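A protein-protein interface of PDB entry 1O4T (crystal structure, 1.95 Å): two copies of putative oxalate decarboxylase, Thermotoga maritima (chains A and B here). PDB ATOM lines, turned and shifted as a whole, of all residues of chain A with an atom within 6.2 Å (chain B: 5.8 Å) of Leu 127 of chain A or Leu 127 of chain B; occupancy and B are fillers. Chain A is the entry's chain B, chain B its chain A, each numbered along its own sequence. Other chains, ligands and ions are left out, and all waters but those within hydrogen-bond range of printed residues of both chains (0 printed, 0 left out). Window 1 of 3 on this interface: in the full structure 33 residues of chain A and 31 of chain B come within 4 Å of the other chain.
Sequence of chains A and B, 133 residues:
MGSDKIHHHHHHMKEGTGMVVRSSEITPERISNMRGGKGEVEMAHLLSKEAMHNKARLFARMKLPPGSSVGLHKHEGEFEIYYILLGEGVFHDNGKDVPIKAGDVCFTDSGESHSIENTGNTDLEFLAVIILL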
ATOM      1  N   LEU A  46      14.703  -1.043 -10.373  1.00  0.00           N
ATOM      2  CA  LEU A  46      13.977  -0.181 -11.294  1.00  0.00           C
ATOM      3  C   LEU A  46      12.962   0.678 -10.589  1.00  0.00           C
ATOM      4  O   LEU A  46      12.744   1.799 -11.005  1.00  0.00           O
ATOM      5  CB  LEU A  46      13.283  -1.008 -12.379  1.00  0.00           C
ATOM      6  CG  LEU A  46      14.220  -1.842 -13.242  1.00  0.00           C
ATOM      7  CD1 LEU A  46      13.349  -2.669 -14.187  1.00  0.00           C
ATOM      8  CD2 LEU A  46      15.292  -1.091 -13.998  1.00  0.00           C
ATOM      9  N   PHE A  59      11.530  -4.666  -7.778  1.00  0.00           N
ATOM     10  CA  PHE A  59      11.271  -4.632  -9.225  1.00  0.00           C
ATOM     11  C   PHE A  59      12.595  -4.363  -9.933  1.00  0.00           C
ATOM     12  O   PHE A  59      13.039  -3.199 -10.082  1.00  0.00           O
ATOM     13  CB  PHE A  59      10.239  -3.544  -9.602  1.00  0.00           C
ATOM     14  CG  PHE A  59       9.667  -3.697 -10.989  1.00  0.00           C
ATOM     15  CD1 PHE A  59      10.160  -2.983 -12.035  1.00  0.00           C
ATOM     16  CD2 PHE A  59       8.639  -4.598 -11.247  1.00  0.00           C
ATOM     17  CE1 PHE A  59       9.668  -3.146 -13.316  1.00  0.00           C
ATOM     18  CE2 PHE A  59       8.140  -4.760 -12.540  1.00  0.00           C
ATOM     19  CZ  PHE A  59       8.683  -4.028 -13.574  1.00  0.00           C
ATOM     20  N   ALA A  60      13.257  -5.440 -10.340  1.00  0.00           N
ATOM     21  CA  ALA A  60      14.638  -5.360 -10.811  1.00  0.00           C
ATOM     22  C   ALA A  60      14.826  -6.069 -12.133  1.00  0.00           C
ATOM     23  O   ALA A  60      14.060  -6.991 -12.466  1.00  0.00           O
ATOM     24  CB  ALA A  60      15.554  -5.952  -9.763  1.00  0.00           C
ATOM     25  N   ARG A  61      15.832  -5.597 -12.892  1.00  0.00           N
ATOM     26  CA  ARG A  61      16.313  -6.233 -14.106  1.00  0.00           C
ATOM     27  C   ARG A  61      17.673  -6.893 -13.794  1.00  0.00           C
ATOM     28  O   ARG A  61      18.652  -6.223 -13.412  1.00  0.00           O
ATOM     29  CB  ARG A  61      16.477  -5.205 -15.212  1.00  0.00           C
ATOM     30  CG  ARG A  61      16.931  -5.758 -16.558  1.00  0.00           C
ATOM     31  CD  ARG A  61      17.087  -4.665 -17.589  1.00  0.00           C
ATOM     32  NE  ARG A  61      17.653  -5.134 -18.851  1.00  0.00           N
ATOM     33  CZ  ARG A  61      17.860  -4.374 -19.929  1.00  0.00           C
ATOM     34  NH1 ARG A  61      17.508  -3.078 -19.926  1.00  0.00           N
ATOM     35  NH2 ARG A  61      18.431  -4.902 -21.023  1.00  0.00           N
ATOM     36  N   MET A  62      17.718  -8.209 -13.945  1.00  0.00           N
ATOM     37  CA  MET A  62      18.859  -9.029 -13.567  1.00  0.00           C
ATOM     38  C   MET A  62      19.583  -9.418 -14.842  1.00  0.00           C
ATOM     39  O   MET A  62      18.938  -9.596 -15.881  1.00  0.00           O
ATOM     40  CB  MET A  62      18.391 -10.321 -12.906  1.00  0.00           C
ATOM     41  CG  MET A  62      17.476 -10.132 -11.725  1.00  0.00           C
ATOM     42  SD  MET A  62      18.359  -9.476 -10.396  1.00  0.00           S
ATOM     43  CE  MET A  62      19.867 -10.472 -10.337  1.00  0.00           C
ATOM     44  N   ILE A  81       7.908 -13.326  -9.349  1.00  0.00           N
ATOM     45  CA  ILE A  81       7.736 -13.571 -10.766  1.00  0.00           C
ATOM     46  C   ILE A  81       8.992 -13.156 -11.448  1.00  0.00           C
ATOM     47  O   ILE A  81       9.517 -12.096 -11.161  1.00  0.00           O
ATOM     48  CB  ILE A  81       6.600 -12.654 -11.283  1.00  0.00           C
ATOM     49  CG1 ILE A  81       5.295 -12.987 -10.551  1.00  0.00           C
ATOM     50  CG2 ILE A  81       6.425 -12.773 -12.785  1.00  0.00           C
ATOM     51  CD1 ILE A  81       4.264 -11.921 -10.656  1.00  0.00           C
ATOM     52  N   TYR A  82       9.487 -13.999 -12.330  1.00  0.00           N
ATOM     53  CA  TYR A  82      10.514 -13.634 -13.272  1.00  0.00           C
ATOM     54  C   TYR A  82       9.831 -13.608 -14.636  1.00  0.00           C
ATOM     55  O   TYR A  82       9.055 -14.519 -14.995  1.00  0.00           O
ATOM     56  CB  TYR A  82      11.618 -14.659 -13.362  1.00  0.00           C
ATOM     57  CG  TYR A  82      12.479 -14.956 -12.155  1.00  0.00           C
ATOM     58  CD1 TYR A  82      13.174 -16.162 -12.095  1.00  0.00           C
ATOM     59  CD2 TYR A  82      12.644 -14.055 -11.104  1.00  0.00           C
ATOM     60  CE1 TYR A  82      14.005 -16.466 -11.036  1.00  0.00           C
ATOM     61  CE2 TYR A  82      13.496 -14.344 -10.070  1.00  0.00           C
ATOM     62  CZ  TYR A  82      14.167 -15.573 -10.025  1.00  0.00           C
ATOM     63  OH  TYR A  82      15.022 -15.881  -8.982  1.00  0.00           O
ATOM     64  N   TYR A  83      10.110 -12.555 -15.392  1.00  0.00           N
ATOM     65  CA  TYR A  83       9.778 -12.528 -16.796  1.00  0.00           C
ATOM     66  C   TYR A  83      11.117 -12.522 -17.540  1.00  0.00           C
ATOM     67  O   TYR A  83      11.927 -11.561 -17.415  1.00  0.00           O
ATOM     68  CB  TYR A  83       8.954 -11.286 -17.100  1.00  0.00           C
ATOM     69  CG  TYR A  83       8.572 -11.290 -18.514  1.00  0.00           C
ATOM     70  CD1 TYR A  83       7.474 -11.998 -18.930  1.00  0.00           C
ATOM     71  CD2 TYR A  83       9.430 -10.762 -19.483  1.00  0.00           C
ATOM     72  CE1 TYR A  83       7.128 -12.042 -20.252  1.00  0.00           C
ATOM     73  CE2 TYR A  83       9.111 -10.842 -20.835  1.00  0.00           C
ATOM     74  CZ  TYR A  83       7.962 -11.462 -21.212  1.00  0.00           C
ATOM     75  OH  TYR A  83       7.630 -11.570 -22.537  1.00  0.00           O
ATOM     76  N   ILE A  84      11.381 -13.586 -18.299  1.00  0.00           N
ATOM     77  CA  ILE A  84      12.660 -13.722 -19.012  1.00  0.00           C
ATOM     78  C   ILE A  84      12.721 -12.741 -20.232  1.00  0.00           C
ATOM     79  O   ILE A  84      11.861 -12.789 -21.107  1.00  0.00           O
ATOM     80  CB  ILE A  84      12.936 -15.175 -19.460  1.00  0.00           C
ATOM     81  CG1 ILE A  84      12.726 -16.189 -18.315  1.00  0.00           C
ATOM     82  CG2 ILE A  84      14.329 -15.331 -19.973  1.00  0.00           C
ATOM     83  CD1 ILE A  84      13.395 -15.838 -16.990  1.00  0.00           C
ATOM     84  N   LEU A  85      13.770 -11.902 -20.283  1.00  0.00           N
ATOM     85  CA  LEU A  85      13.968 -10.888 -21.358  1.00  0.00           C
ATOM     86  C   LEU A  85      14.787 -11.304 -22.565  1.00  0.00           C
ATOM     87  O   LEU A  85      14.440 -10.982 -23.703  1.00  0.00           O
ATOM     88  CB  LEU A  85      14.550  -9.587 -20.755  1.00  0.00           C
ATOM     89  CG  LEU A  85      13.710  -8.916 -19.653  1.00  0.00           C
ATOM     90  CD1 LEU A  85      14.533  -7.824 -18.922  1.00  0.00           C
ATOM     91  CD2 LEU A  85      12.391  -8.367 -20.254  1.00  0.00           C
ATOM     92  N   GLU A 125      18.891 -12.408 -19.263  1.00  0.00           N
ATOM     93  CA  GLU A 125      18.295 -11.248 -18.575  1.00  0.00           C
ATOM     94  C   GLU A 125      16.849 -11.474 -18.266  1.00  0.00           C
ATOM     95  O   GLU A 125      16.119 -12.175 -18.981  1.00  0.00           O
ATOM     96  CB  GLU A 125      18.443  -9.987 -19.381  1.00  0.00           C
ATOM     97  CG  GLU A 125      19.867  -9.651 -19.665  1.00  0.00           C
ATOM     98  CD  GLU A 125      20.022  -8.268 -20.240  1.00  0.00           C
ATOM     99  OE1 GLU A 125      19.038  -7.506 -20.256  1.00  0.00           O
ATOM    100  OE2 GLU A 125      21.121  -7.958 -20.695  1.00  0.00           O
ATOM    101  N   PHE A 126      16.447 -10.954 -17.130  1.00  0.00           N
ATOM    102  CA  PHE A 126      15.067 -11.112 -16.667  1.00  0.00           C
ATOM    103  C   PHE A 126      14.674 -10.079 -15.646  1.00  0.00           C
ATOM    104  O   PHE A 126      15.526  -9.532 -14.912  1.00  0.00           O
ATOM    105  CB  PHE A 126      14.813 -12.505 -16.118  1.00  0.00           C
ATOM    106  CG  PHE A 126      15.638 -12.882 -14.906  1.00  0.00           C
ATOM    107  CD1 PHE A 126      15.116 -12.757 -13.630  1.00  0.00           C
ATOM    108  CD2 PHE A 126      16.885 -13.504 -15.062  1.00  0.00           C
ATOM    109  CE1 PHE A 126      15.864 -13.140 -12.506  1.00  0.00           C
ATOM    110  CE2 PHE A 126      17.616 -13.918 -13.968  1.00  0.00           C
ATOM    111  CZ  PHE A 126      17.097 -13.714 -12.668  1.00  0.00           C
ATOM    112  N   LEU A 127      13.373  -9.830 -15.623  1.00  0.00           N
ATOM    113  CA  LEU A 127      12.744  -9.023 -14.635  1.00  0.00           C
ATOM    114  C   LEU A 127      12.435  -9.910 -13.454  1.00  0.00           C
ATOM    115  O   LEU A 127      12.068 -11.070 -13.619  1.00  0.00           O
ATOM    116  CB  LEU A 127      11.437  -8.452 -15.161  1.00  0.00           C
ATOM    117  CG  LEU A 127      11.370  -7.004 -15.639  1.00  0.00           C
ATOM    118  CD1 LEU A 127      12.658  -6.466 -16.241  1.00  0.00           C
ATOM    119  CD2 LEU A 127      10.171  -6.827 -16.582  1.00  0.00           C
ATOM    120  N   ALA A 128      12.557  -9.346 -12.257  1.00  0.00           N
ATOM    121  CA  ALA A 128      12.143 -10.032 -11.057  1.00  0.00           C
ATOM    122  C   ALA A 128      11.263  -9.104 -10.240  1.00  0.00           C
ATOM    123  O   ALA A 128      11.649  -7.933  -9.979  1.00  0.00           O
ATOM    124  CB  ALA A 128      13.363 -10.472 -10.265  1.00  0.00           C
ATOM    125  N   VAL A 129      10.091  -9.588  -9.833  1.00  0.00           N
ATOM    126  CA  VAL A 129       9.209  -8.800  -8.994  1.00  0.00           C
ATOM    127  C   VAL A 129       8.726  -9.623  -7.853  1.00  0.00           C
ATOM    128  O   VAL A 129       8.218 -10.729  -8.047  1.00  0.00           O
ATOM    129  CB  VAL A 129       8.008  -8.183  -9.827  1.00  0.00           C
ATOM    130  CG1 VAL A 129       7.130  -9.197 -10.379  1.00  0.00           C
ATOM    131  CG2 VAL A 129       7.204  -7.259  -9.021  1.00  0.00           C
ATOM    132  N   LEU B  46      -0.862 -13.398 -18.714  1.00  0.00           N
ATOM    133  CA  LEU B  46       0.204 -14.342 -18.379  1.00  0.00           C
ATOM    134  C   LEU B  46      -0.026 -15.030 -17.028  1.00  0.00           C
ATOM    135  O   LEU B  46       0.254 -16.225 -16.886  1.00  0.00           O
ATOM    136  CB  LEU B  46       1.546 -13.622 -18.421  1.00  0.00           C
ATOM    137  CG  LEU B  46       1.789 -12.954 -19.750  1.00  0.00           C
ATOM    138  CD1 LEU B  46       3.161 -12.324 -19.702  1.00  0.00           C
ATOM    139  CD2 LEU B  46       1.653 -13.895 -20.918  1.00  0.00           C
ATOM    140  N   PHE B  59      -1.356  -9.052 -15.252  1.00  0.00           N
ATOM    141  CA  PHE B  59       0.033  -9.302 -15.590  1.00  0.00           C
ATOM    142  C   PHE B  59       0.007  -9.799 -17.039  1.00  0.00           C
ATOM    143  O   PHE B  59      -0.256 -10.967 -17.291  1.00  0.00           O
ATOM    144  CB  PHE B  59       0.695 -10.298 -14.626  1.00  0.00           C
ATOM    145  CG  PHE B  59       2.185 -10.382 -14.776  1.00  0.00           C
ATOM    146  CD1 PHE B  59       2.747 -11.104 -15.814  1.00  0.00           C
ATOM    147  CD2 PHE B  59       3.028  -9.674 -13.943  1.00  0.00           C
ATOM    148  CE1 PHE B  59       4.128 -11.173 -16.010  1.00  0.00           C
ATOM    149  CE2 PHE B  59       4.418  -9.705 -14.141  1.00  0.00           C
ATOM    150  CZ  PHE B  59       4.969 -10.459 -15.200  1.00  0.00           C
ATOM    151  N   ALA B  60       0.233  -8.885 -17.995  1.00  0.00           N
ATOM    152  CA  ALA B  60      -0.044  -9.149 -19.385  1.00  0.00           C
ATOM    153  C   ALA B  60       1.024  -8.608 -20.275  1.00  0.00           C
ATOM    154  O   ALA B  60       1.706  -7.649 -19.924  1.00  0.00           O
ATOM    155  CB  ALA B  60      -1.343  -8.523 -19.781  1.00  0.00           C
ATOM    156  N   ARG B  61       1.156  -9.233 -21.435  1.00  0.00           N
ATOM    157  CA  ARG B  61       2.033  -8.749 -22.493  1.00  0.00           C
ATOM    158  C   ARG B  61       1.159  -8.112 -23.580  1.00  0.00           C
ATOM    159  O   ARG B  61       0.206  -8.769 -24.094  1.00  0.00           O
ATOM    160  CB  ARG B  61       2.837  -9.898 -23.082  1.00  0.00           C
ATOM    161  CG  ARG B  61       3.953  -9.456 -23.975  1.00  0.00           C
ATOM    162  CD  ARG B  61       4.710 -10.579 -24.676  1.00  0.00           C
ATOM    163  NE  ARG B  61       5.710  -9.994 -25.587  1.00  0.00           N
ATOM    164  CZ  ARG B  61       6.749 -10.650 -26.114  1.00  0.00           C
ATOM    165  NH1 ARG B  61       6.951 -11.939 -25.848  1.00  0.00           N
ATOM    166  NH2 ARG B  61       7.598 -10.010 -26.913  1.00  0.00           N
ATOM    167  N   MET B  62       1.439  -6.852 -23.913  1.00  0.00           N
ATOM    168  CA  MET B  62       0.627  -6.116 -24.881  1.00  0.00           C
ATOM    169  C   MET B  62       1.458  -5.978 -26.135  1.00  0.00           C
ATOM    170  O   MET B  62       2.653  -5.828 -26.015  1.00  0.00           O
ATOM    171  CB  MET B  62       0.371  -4.719 -24.378  1.00  0.00           C
ATOM    172  CG  MET B  62      -0.305  -4.647 -23.013  1.00  0.00           C
ATOM    173  SD  MET B  62      -1.896  -5.264 -23.127  1.00  0.00           S
ATOM    174  CE  MET B  62      -2.536  -4.222 -24.485  1.00  0.00           C
ATOM    175  N   ILE B  81       2.434  -0.492 -13.924  1.00  0.00           N
ATOM    176  CA  ILE B  81       3.779  -0.415 -14.429  1.00  0.00           C
ATOM    177  C   ILE B  81       3.774  -0.996 -15.843  1.00  0.00           C
ATOM    178  O   ILE B  81       3.269  -2.081 -16.071  1.00  0.00           O
ATOM    179  CB  ILE B  81       4.736  -1.263 -13.544  1.00  0.00           C
ATOM    180  CG1 ILE B  81       4.623  -0.868 -12.068  1.00  0.00           C
ATOM    181  CG2 ILE B  81       6.194  -1.165 -14.063  1.00  0.00           C
ATOM    182  CD1 ILE B  81       5.138  -1.975 -11.156  1.00  0.00           C
ATOM    183  N   TYR B  82       4.334  -0.278 -16.803  1.00  0.00           N
ATOM    184  CA  TYR B  82       4.716  -0.876 -18.057  1.00  0.00           C
ATOM    185  C   TYR B  82       6.238  -1.093 -18.089  1.00  0.00           C
ATOM    186  O   TYR B  82       7.017  -0.214 -17.687  1.00  0.00           O
ATOM    187  CB  TYR B  82       4.386   0.051 -19.209  1.00  0.00           C
ATOM    188  CG  TYR B  82       2.943   0.442 -19.482  1.00  0.00           C
ATOM    189  CD1 TYR B  82       2.662   1.559 -20.267  1.00  0.00           C
ATOM    190  CD2 TYR B  82       1.863  -0.307 -19.004  1.00  0.00           C
ATOM    191  CE1 TYR B  82       1.376   1.898 -20.583  1.00  0.00           C
ATOM    192  CE2 TYR B  82       0.580   0.027 -19.321  1.00  0.00           C
ATOM    193  CZ  TYR B  82       0.325   1.141 -20.102  1.00  0.00           C
ATOM    194  OH  TYR B  82      -1.001   1.483 -20.387  1.00  0.00           O
ATOM    195  N   TYR B  83       6.672  -2.262 -18.563  1.00  0.00           N
ATOM    196  CA  TYR B  83       8.058  -2.469 -18.984  1.00  0.00           C
ATOM    197  C   TYR B  83       8.098  -2.666 -20.517  1.00  0.00           C
ATOM    198  O   TYR B  83       7.531  -3.620 -21.084  1.00  0.00           O
ATOM    199  CB  TYR B  83       8.703  -3.639 -18.239  1.00  0.00           C
ATOM    200  CG  TYR B  83      10.169  -3.771 -18.588  1.00  0.00           C
ATOM    201  CD1 TYR B  83      11.141  -3.164 -17.811  1.00  0.00           C
ATOM    202  CD2 TYR B  83      10.571  -4.469 -19.698  1.00  0.00           C
ATOM    203  CE1 TYR B  83      12.506  -3.218 -18.160  1.00  0.00           C
ATOM    204  CE2 TYR B  83      11.935  -4.563 -20.058  1.00  0.00           C
ATOM    205  CZ  TYR B  83      12.906  -3.929 -19.265  1.00  0.00           C
ATOM    206  OH  TYR B  83      14.240  -3.989 -19.605  1.00  0.00           O
ATOM    207  N   ILE B  84       8.753  -1.740 -21.201  1.00  0.00           N
ATOM    208  CA  ILE B  84       8.787  -1.768 -22.658  1.00  0.00           C
ATOM    209  C   ILE B  84       9.765  -2.835 -23.128  1.00  0.00           C
ATOM    210  O   ILE B  84      10.969  -2.773 -22.822  1.00  0.00           O
ATOM    211  CB  ILE B  84       9.186  -0.383 -23.235  1.00  0.00           C
ATOM    212  CG1 ILE B  84       8.375   0.760 -22.615  1.00  0.00           C
ATOM    213  CG2 ILE B  84       9.070  -0.373 -24.788  1.00  0.00           C
ATOM    214  CD1 ILE B  84       6.848   0.553 -22.670  1.00  0.00           C
ATOM    215  N   LEU B  85       9.248  -3.788 -23.911  1.00  0.00           N
ATOM    216  CA  LEU B  85      10.026  -4.933 -24.384  1.00  0.00           C
ATOM    217  C   LEU B  85      10.616  -4.784 -25.790  1.00  0.00           C
ATOM    218  O   LEU B  85      11.724  -5.269 -26.028  1.00  0.00           O
ATOM    219  CB  LEU B  85       9.161  -6.208 -24.376  1.00  0.00           C
ATOM    220  CG  LEU B  85       8.513  -6.720 -23.110  1.00  0.00           C
ATOM    221  CD1 LEU B  85       7.509  -7.783 -23.474  1.00  0.00           C
ATOM    222  CD2 LEU B  85       9.550  -7.278 -22.219  1.00  0.00           C
ATOM    223  N   GLU B 125       5.917  -3.686 -28.056  1.00  0.00           N
ATOM    224  CA  GLU B 125       5.413  -4.615 -27.063  1.00  0.00           C
ATOM    225  C   GLU B 125       5.875  -4.228 -25.679  1.00  0.00           C
ATOM    226  O   GLU B 125       6.965  -3.700 -25.493  1.00  0.00           O
ATOM    227  CB  GLU B 125       5.872  -6.012 -27.384  1.00  0.00           C
ATOM    228  CG  GLU B 125       5.647  -6.409 -28.830  1.00  0.00           C
ATOM    229  CD  GLU B 125       5.546  -7.914 -29.042  1.00  0.00           C
ATOM    230  OE1 GLU B 125       5.314  -8.621 -28.055  1.00  0.00           O
ATOM    231  OE2 GLU B 125       5.646  -8.377 -30.211  1.00  0.00           O
ATOM    232  N   PHE B 126       5.040  -4.505 -24.689  1.00  0.00           N
ATOM    233  CA  PHE B 126       5.397  -4.233 -23.331  1.00  0.00           C
ATOM    234  C   PHE B 126       4.622  -5.110 -22.363  1.00  0.00           C
ATOM    235  O   PHE B 126       3.532  -5.637 -22.672  1.00  0.00           O
ATOM    236  CB  PHE B 126       5.173  -2.758 -22.992  1.00  0.00           C
ATOM    237  CG  PHE B 126       3.770  -2.254 -23.254  1.00  0.00           C
ATOM    238  CD1 PHE B 126       2.846  -2.178 -22.237  1.00  0.00           C
ATOM    239  CD2 PHE B 126       3.410  -1.803 -24.522  1.00  0.00           C
ATOM    240  CE1 PHE B 126       1.547  -1.714 -22.498  1.00  0.00           C
ATOM    241  CE2 PHE B 126       2.147  -1.310 -24.791  1.00  0.00           C
ATOM    242  CZ  PHE B 126       1.217  -1.248 -23.768  1.00  0.00           C
ATOM    243  N   LEU B 127       5.194  -5.231 -21.187  1.00  0.00           N
ATOM    244  CA  LEU B 127       4.552  -5.862 -20.062  1.00  0.00           C
ATOM    245  C   LEU B 127       3.742  -4.875 -19.266  1.00  0.00           C
ATOM    246  O   LEU B 127       4.208  -3.787 -19.008  1.00  0.00           O
ATOM    247  CB  LEU B 127       5.662  -6.416 -19.178  1.00  0.00           C
ATOM    248  CG  LEU B 127       5.573  -7.844 -18.765  1.00  0.00           C
ATOM    249  CD1 LEU B 127       5.498  -8.766 -19.982  1.00  0.00           C
ATOM    250  CD2 LEU B 127       6.819  -8.104 -17.855  1.00  0.00           C
ATOM    251  N   ALA B 128       2.547  -5.260 -18.836  1.00  0.00           N
ATOM    252  CA  ALA B 128       1.672  -4.404 -18.011  1.00  0.00           C
ATOM    253  C   ALA B 128       1.286  -5.144 -16.750  1.00  0.00           C
ATOM    254  O   ALA B 128       0.789  -6.268 -16.823  1.00  0.00           O
ATOM    255  CB  ALA B 128       0.459  -4.004 -18.782  1.00  0.00           C
ATOM    256  N   VAL B 129       1.477  -4.508 -15.598  1.00  0.00           N
ATOM    257  CA  VAL B 129       1.180  -5.113 -14.326  1.00  0.00           C
ATOM    258  C   VAL B 129       0.365  -4.112 -13.481  1.00  0.00           C
ATOM    259  O   VAL B 129       0.804  -3.013 -13.244  1.00  0.00           O
ATOM    260  CB  VAL B 129       2.466  -5.453 -13.537  1.00  0.00           C
ATOM    261  CG1 VAL B 129       2.135  -6.389 -12.391  1.00  0.00           C
ATOM    262  CG2 VAL B 129       3.466  -6.104 -14.444  1.00  0.00           C
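The guanidinium group (NH1) of Arg 61 of chain B is in hydrogen-bond range of the side-chain hydroxyl (OH) of Tyr 83 of chain A.
The side-chain hydroxyl (OH) of Tyr 83 of chain B sits at hydrogen-bond distance from the guanidinium group (NH1) of Arg 61 of chain A (3.4 Å).
O of Phe 59 of chain B sits at hydrogen-bond distance from N of Leu 46 of chain B (2.9 Å).
The guanidinium group (NE) of Arg 61 of chain B is in salt-bridge range of the side-chain carboxylate (OE1) of Glu 125 of chain B, at 2.9 Å.
The backbone NH (N) of Val 129 of chain B lies within hydrogen-bond range of the backbone carbonyl oxygen (O) of Ile 81 of chain B.
O of Tyr 83 of chain B is in hydrogen-bond range of N of Leu 127 of chain B.
The backbone NH (N) of Val 129 of chain A sits at hydrogen-bond distance from the backbone carbonyl oxygen (O) of Ile 81 of chain A (2.9 Å).
The backbone carbonyl oxygen (O) of Tyr 83 of chain A is in hydrogen-bond range of the backbone NH (N) of Leu 127 of chain A (2.9 Å).
CZ of Phe 59 of chain A touches CG2 of Ile 81 of chain B (3.8 Å).
Phe 59 of chain B touches Ile 81 of chain A (CZ to CG2, 3.6 Å).
CE2 of Tyr 83 of chain A touches CD2 of Leu 85 of chain B (3.8 Å).
Tyr 83 of chain A touches Leu 127 of chain B.
Tyr 83 of chain B touches Leu 85 of chain A.
Leu 85 of chain A touches Leu 85 of chain B.
Leu 127 of chain A touches Tyr 83 of chain B (CD2 to CG, 3.7 Å).
Leu 127 of chain A touches Leu 127 of chain B.
Of the printed residues of chain B, Leu 85 of chain A touches Tyr 83 (3.8 Å) and Leu 85 (3.6 Å).
Of the printed residues of chain B, Leu 127 of chain A touches Tyr 83 and Leu 127.
Of the printed residues of chain A, Phe 59 of chain B touches Ile 81.
Of the printed residues of chain A, Leu 85 of chain B touches Tyr 83 (3.8 Å) and Leu 85 (3.6 Å).
Leu 127 of chain B touches just these residues of chain A: Tyr 83 and Leu 127.
The nearest residue of chain B that does not touch Leu 127 of chain A is Leu 85 of chain B (5.7 Å).
Of the 15 printed residues of chain B, 6 touch a printed residue of chain A.
Printed residues of chain B that touch a printed residue of chain A: Phe 59, Arg 61, Ile 81, Tyr 83, Leu 85 and Leu 127.
Phe 59 of chain A touches Ile 81 of chain B, and with the chains exchanged Ile 81 of chain A touches Phe 59 of chain B.
Arg 61 of chain A touches Tyr 83 of chain B, and with the chains exchanged Tyr 83 of chain A touches Arg 61 of chain B.
Tyr 83 of chain A touches Leu 127 of chain B, and with the chains exchanged Leu 127 of chain A touches Tyr 83 of chain B.
Leu 127 of chain B touches its own counterpart, Leu 127 of chain A.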
